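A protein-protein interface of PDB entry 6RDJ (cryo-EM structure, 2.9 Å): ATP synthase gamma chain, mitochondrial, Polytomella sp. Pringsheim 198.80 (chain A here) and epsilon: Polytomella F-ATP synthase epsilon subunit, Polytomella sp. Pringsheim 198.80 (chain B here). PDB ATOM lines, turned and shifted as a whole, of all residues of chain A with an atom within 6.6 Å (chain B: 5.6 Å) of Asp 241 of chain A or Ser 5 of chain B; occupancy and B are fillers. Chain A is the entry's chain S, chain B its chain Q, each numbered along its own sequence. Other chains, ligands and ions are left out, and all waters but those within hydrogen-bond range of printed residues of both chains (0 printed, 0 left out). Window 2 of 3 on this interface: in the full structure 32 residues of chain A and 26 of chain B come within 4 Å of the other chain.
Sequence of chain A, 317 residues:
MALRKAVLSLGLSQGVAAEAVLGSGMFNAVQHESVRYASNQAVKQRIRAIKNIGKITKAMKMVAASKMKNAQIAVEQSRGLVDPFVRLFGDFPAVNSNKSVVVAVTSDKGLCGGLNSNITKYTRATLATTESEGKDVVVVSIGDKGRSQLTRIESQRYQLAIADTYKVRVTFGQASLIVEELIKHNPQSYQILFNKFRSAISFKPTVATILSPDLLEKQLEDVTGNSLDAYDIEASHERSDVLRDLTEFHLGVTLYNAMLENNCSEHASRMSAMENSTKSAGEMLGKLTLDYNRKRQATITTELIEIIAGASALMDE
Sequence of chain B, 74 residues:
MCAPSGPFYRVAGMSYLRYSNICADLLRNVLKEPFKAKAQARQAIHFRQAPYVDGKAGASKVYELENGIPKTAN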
ATOM      1  N   ALA A 235     -14.976 -16.374 -20.438  1.00  0.00           N
ATOM      2  CA  ALA A 235     -14.463 -17.480 -21.227  1.00  0.00           C
ATOM      3  C   ALA A 235     -12.975 -17.628 -20.983  1.00  0.00           C
ATOM      4  O   ALA A 235     -12.356 -16.841 -20.267  1.00  0.00           O
ATOM      5  CB  ALA A 235     -14.739 -17.264 -22.710  1.00  0.00           C
ATOM      6  N   HIS A 237     -10.416 -17.854 -23.595  1.00  0.00           N
ATOM      7  CA  HIS A 237      -9.694 -17.010 -24.530  1.00  0.00           C
ATOM      8  C   HIS A 237     -10.467 -15.710 -24.751  1.00  0.00           C
ATOM      9  O   HIS A 237     -11.323 -15.338 -23.946  1.00  0.00           O
ATOM     10  CB  HIS A 237      -9.416 -17.800 -25.800  1.00  0.00           C
ATOM     11  CG  HIS A 237      -8.432 -18.904 -25.595  1.00  0.00           C
ATOM     12  ND1 HIS A 237      -8.705 -20.003 -24.812  1.00  0.00           N
ATOM     13  CD2 HIS A 237      -7.171 -19.069 -26.049  1.00  0.00           C
ATOM     14  CE1 HIS A 237      -7.656 -20.805 -24.801  1.00  0.00           C
ATOM     15  NE2 HIS A 237      -6.711 -20.261 -25.545  1.00  0.00           N
ATOM     16  N   GLU A 238     -10.134 -14.982 -25.810  1.00  0.00           N
ATOM     17  CA  GLU A 238     -10.607 -13.623 -26.010  1.00  0.00           C
ATOM     18  C   GLU A 238     -12.088 -13.575 -26.365  1.00  0.00           C
ATOM     19  O   GLU A 238     -12.743 -14.593 -26.589  1.00  0.00           O
ATOM     20  CB  GLU A 238      -9.785 -12.941 -27.098  1.00  0.00           C
ATOM     21  CG  GLU A 238      -8.418 -12.557 -26.612  1.00  0.00           C
ATOM     22  CD  GLU A 238      -8.487 -11.432 -25.599  1.00  0.00           C
ATOM     23  OE1 GLU A 238      -9.303 -10.506 -25.793  1.00  0.00           O
ATOM     24  OE2 GLU A 238      -7.765 -11.493 -24.586  1.00  0.00           O
ATOM     25  N   ARG A 239     -12.609 -12.347 -26.414  1.00  0.00           N
ATOM     26  CA  ARG A 239     -14.012 -12.137 -26.737  1.00  0.00           C
ATOM     27  C   ARG A 239     -14.304 -12.420 -28.201  1.00  0.00           C
ATOM     28  O   ARG A 239     -15.440 -12.763 -28.546  1.00  0.00           O
ATOM     29  CB  ARG A 239     -14.425 -10.714 -26.390  1.00  0.00           C
ATOM     30  CG  ARG A 239     -15.907 -10.561 -26.215  1.00  0.00           C
ATOM     31  CD  ARG A 239     -16.285  -9.167 -25.835  1.00  0.00           C
ATOM     32  NE  ARG A 239     -15.894  -8.211 -26.850  1.00  0.00           N
ATOM     33  CZ  ARG A 239     -16.244  -6.938 -26.818  1.00  0.00           C
ATOM     34  NH1 ARG A 239     -16.990  -6.490 -25.822  1.00  0.00           N
ATOM     35  NH2 ARG A 239     -15.851  -6.118 -27.771  1.00  0.00           N
ATOM     36  N   SER A 240     -13.308 -12.276 -29.073  1.00  0.00           N
ATOM     37  CA  SER A 240     -13.487 -12.664 -30.465  1.00  0.00           C
ATOM     38  C   SER A 240     -13.719 -14.161 -30.587  1.00  0.00           C
ATOM     39  O   SER A 240     -14.559 -14.602 -31.374  1.00  0.00           O
ATOM     40  CB  SER A 240     -12.278 -12.239 -31.288  1.00  0.00           C
ATOM     41  OG  SER A 240     -11.124 -12.957 -30.896  1.00  0.00           O
ATOM     42  N   ASP A 241     -13.025 -14.954 -29.777  1.00  0.00           N
ATOM     43  CA  ASP A 241     -13.237 -16.392 -29.773  1.00  0.00           C
ATOM     44  C   ASP A 241     -14.561 -16.788 -29.145  1.00  0.00           C
ATOM     45  O   ASP A 241     -15.197 -17.730 -29.628  1.00  0.00           O
ATOM     46  CB  ASP A 241     -12.093 -17.087 -29.045  1.00  0.00           C
ATOM     47  CG  ASP A 241     -10.739 -16.684 -29.579  1.00  0.00           C
ATOM     48  OD1 ASP A 241      -9.897 -16.210 -28.790  1.00  0.00           O
ATOM     49  OD2 ASP A 241     -10.513 -16.837 -30.796  1.00  0.00           O
ATOM     50  N   VAL A 242     -15.010 -16.083 -28.105  1.00  0.00           N
ATOM     51  CA  VAL A 242     -16.281 -16.450 -27.499  1.00  0.00           C
ATOM     52  C   VAL A 242     -17.434 -16.026 -28.396  1.00  0.00           C
ATOM     53  O   VAL A 242     -18.451 -16.711 -28.466  1.00  0.00           O
ATOM     54  CB  VAL A 242     -16.405 -15.893 -26.061  1.00  0.00           C
ATOM     55  CG1 VAL A 242     -16.816 -14.445 -26.003  1.00  0.00           C
ATOM     56  CG2 VAL A 242     -17.376 -16.687 -25.284  1.00  0.00           C
ATOM     57  N   LEU A 243     -17.265 -14.955 -29.175  1.00  0.00           N
ATOM     58  CA  LEU A 243     -18.285 -14.595 -30.147  1.00  0.00           C
ATOM     59  C   LEU A 243     -18.248 -15.509 -31.359  1.00  0.00           C
ATOM     60  O   LEU A 243     -19.290 -15.776 -31.961  1.00  0.00           O
ATOM     61  CB  LEU A 243     -18.114 -13.143 -30.566  1.00  0.00           C
ATOM     62  CG  LEU A 243     -19.082 -12.140 -29.955  1.00  0.00           C
ATOM     63  CD1 LEU A 243     -18.896 -12.030 -28.474  1.00  0.00           C
ATOM     64  CD2 LEU A 243     -18.853 -10.805 -30.597  1.00  0.00           C
ATOM     65  N   ARG A 244     -17.065 -16.000 -31.723  1.00  0.00           N
ATOM     66  CA  ARG A 244     -16.950 -16.963 -32.807  1.00  0.00           C
ATOM     67  C   ARG A 244     -17.607 -18.285 -32.436  1.00  0.00           C
ATOM     68  O   ARG A 244     -18.210 -18.941 -33.288  1.00  0.00           O
ATOM     69  CB  ARG A 244     -15.473 -17.148 -33.159  1.00  0.00           C
ATOM     70  CG  ARG A 244     -15.161 -18.211 -34.178  1.00  0.00           C
ATOM     71  CD  ARG A 244     -15.693 -17.834 -35.534  1.00  0.00           C
ATOM     72  NE  ARG A 244     -14.948 -16.736 -36.128  1.00  0.00           N
ATOM     73  CZ  ARG A 244     -15.130 -16.303 -37.372  1.00  0.00           C
ATOM     74  NH1 ARG A 244     -14.412 -15.291 -37.840  1.00  0.00           N
ATOM     75  NH2 ARG A 244     -16.036 -16.880 -38.144  1.00  0.00           N
ATOM     76  N   ASP A 245     -17.524 -18.685 -31.170  1.00  0.00           N
ATOM     77  CA  ASP A 245     -18.255 -19.868 -30.729  1.00  0.00           C
ATOM     78  C   ASP A 245     -19.746 -19.590 -30.601  1.00  0.00           C
ATOM     79  O   ASP A 245     -20.581 -20.434 -30.953  1.00  0.00           O
ATOM     80  CB  ASP A 245     -17.702 -20.360 -29.398  1.00  0.00           C
ATOM     81  CG  ASP A 245     -16.230 -20.683 -29.466  1.00  0.00           C
ATOM     82  OD1 ASP A 245     -15.658 -21.086 -28.434  1.00  0.00           O
ATOM     83  OD2 ASP A 245     -15.634 -20.526 -30.550  1.00  0.00           O
ATOM     84  N   LEU A 246     -20.091 -18.394 -30.136  1.00  0.00           N
ATOM     85  CA  LEU A 246     -21.464 -18.055 -29.821  1.00  0.00           C
ATOM     86  C   LEU A 246     -22.305 -17.860 -31.070  1.00  0.00           C
ATOM     87  O   LEU A 246     -23.489 -18.184 -31.059  1.00  0.00           O
ATOM     88  CB  LEU A 246     -21.462 -16.798 -28.964  1.00  0.00           C
ATOM     89  CG  LEU A 246     -22.596 -16.535 -28.000  1.00  0.00           C
ATOM     90  CD1 LEU A 246     -22.748 -17.733 -27.141  1.00  0.00           C
ATOM     91  CD2 LEU A 246     -22.213 -15.364 -27.152  1.00  0.00           C
ATOM     92  N   ALA B   3      -2.289 -23.398 -36.383  1.00  0.00           N
ATOM     93  CA  ALA B   3      -2.580 -22.213 -37.189  1.00  0.00           C
ATOM     94  C   ALA B   3      -3.779 -21.343 -36.722  1.00  0.00           C
ATOM     95  O   ALA B   3      -3.702 -20.124 -36.863  1.00  0.00           O
ATOM     96  CB  ALA B   3      -2.755 -22.616 -38.664  1.00  0.00           C
ATOM     97  N   PRO B   4      -4.871 -21.905 -36.183  1.00  0.00           N
ATOM     98  CA  PRO B   4      -5.821 -21.051 -35.469  1.00  0.00           C
ATOM     99  C   PRO B   4      -5.407 -20.831 -34.021  1.00  0.00           C
ATOM    100  O   PRO B   4      -4.704 -21.638 -33.411  1.00  0.00           O
ATOM    101  CB  PRO B   4      -7.140 -21.836 -35.544  1.00  0.00           C
ATOM    102  CG  PRO B   4      -6.928 -22.869 -36.568  1.00  0.00           C
ATOM    103  CD  PRO B   4      -5.500 -23.219 -36.430  1.00  0.00           C
ATOM    104  N   SER B   5      -5.875 -19.713 -33.473  1.00  0.00           N
ATOM    105  CA  SER B   5      -5.515 -19.287 -32.123  1.00  0.00           C
ATOM    106  C   SER B   5      -6.795 -19.065 -31.329  1.00  0.00           C
ATOM    107  O   SER B   5      -7.475 -18.052 -31.509  1.00  0.00           O
ATOM    108  CB  SER B   5      -4.674 -18.022 -32.157  1.00  0.00           C
ATOM    109  OG  SER B   5      -5.437 -16.929 -32.627  1.00  0.00           O
ATOM    110  N   GLY B   6      -7.110 -19.998 -30.448  1.00  0.00           N
ATOM    111  CA  GLY B   6      -8.259 -19.870 -29.591  1.00  0.00           C
ATOM    112  C   GLY B   6      -8.311 -21.009 -28.604  1.00  0.00           C
ATOM    113  O   GLY B   6      -7.284 -21.470 -28.105  1.00  0.00           O
ATOM    114  N   PRO B   7      -9.512 -21.490 -28.306  1.00  0.00           N
ATOM    115  CA  PRO B   7      -9.646 -22.658 -27.432  1.00  0.00           C
ATOM    116  C   PRO B   7      -9.180 -23.916 -28.141  1.00  0.00           C
ATOM    117  O   PRO B   7      -8.966 -23.930 -29.348  1.00  0.00           O
ATOM    118  CB  PRO B   7     -11.139 -22.700 -27.134  1.00  0.00           C
ATOM    119  CG  PRO B   7     -11.647 -21.341 -27.495  1.00  0.00           C
ATOM    120  CD  PRO B   7     -10.814 -20.897 -28.628  1.00  0.00           C
ATOM    121  N   ARG B  10     -10.760 -25.099 -31.198  1.00  0.00           N
ATOM    122  CA  ARG B  10     -10.541 -24.214 -32.331  1.00  0.00           C
ATOM    123  C   ARG B  10      -9.144 -24.378 -32.907  1.00  0.00           C
ATOM    124  O   ARG B  10      -8.958 -24.226 -34.118  1.00  0.00           O
ATOM    125  CB  ARG B  10     -10.777 -22.770 -31.904  1.00  0.00           C
ATOM    126  CG  ARG B  10     -10.902 -21.800 -33.037  1.00  0.00           C
ATOM    127  CD  ARG B  10     -12.165 -22.056 -33.821  1.00  0.00           C
ATOM    128  NE  ARG B  10     -13.362 -21.880 -33.010  1.00  0.00           N
ATOM    129  CZ  ARG B  10     -14.588 -21.807 -33.513  1.00  0.00           C
ATOM    130  NH1 ARG B  10     -14.768 -21.888 -34.821  1.00  0.00           N
ATOM    131  NH2 ARG B  10     -15.627 -21.642 -32.716  1.00  0.00           N
ATOM    132  N   VAL B  11      -8.157 -24.688 -32.062  1.00  0.00           N
ATOM    133  CA  VAL B  11      -6.805 -24.942 -32.548  1.00  0.00           C
ATOM    134  C   VAL B  11      -6.758 -26.223 -33.362  1.00  0.00           C
ATOM    135  O   VAL B  11      -6.074 -26.291 -34.389  1.00  0.00           O
ATOM    136  CB  VAL B  11      -5.809 -24.981 -31.375  1.00  0.00           C
ATOM    137  CG1 VAL B  11      -4.386 -25.047 -31.884  1.00  0.00           C
ATOM    138  CG2 VAL B  11      -5.957 -23.747 -30.529  1.00  0.00           C
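NE2 of His 237 of chain A sits at hydrogen-bond distance from O of Gly 6 of chain B, at 2.9 Å. The side-chain carboxylate (OD2) of Asp 245 of chain A is in salt-bridge range of the guanidinium group (NH2) of Arg 10 of chain B (2.4 Å). The side-chain carboxylate (OD2) of Asp 241 of chain A lies close to the backbone carbonyl oxygen (O) of Ser 5 of chain B, 3.3 Å away.
N of Glu 238 of chain A sits at hydrogen-bond distance from OD1 of Asp 241 of chain A (3.2 Å).
Among the printed residues, merely in contact across the chains: His 237 of chain A with Pro 7 of chain B (3.8 Å), Asp 241 of chain A with Gly 6 of chain B (3.97 Å) and Arg 244 of chain A with Arg 10 of chain B (3.7 Å).
Of the printed residues of chain B, His 237 of chain A touches Gly 6 and Pro 7. Asp 241 of chain A touches two residues of chain B. Printed residues of chain B within 4 Å of Arg 244 of chain A: Arg 10 (3.7 Å). Of the printed residues of chain B, Asp 245 of chain A touches Arg 10. Of chain A, only Asp 241 (3.3 Å) comes within 4 Å of Ser 5 of chain B. Printed residues of chain A within 4 Å of Pro 7 of chain B: His 237 (3.8 Å). The nearest residue of chain B that does not touch Asp 241 of chain A is Pro 7 of chain B (4.04 Å).
Of the 11 printed residues of chain A, 4 touch a printed residue of chain B. Among the printed residues, 6 pairs touch across the chains.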
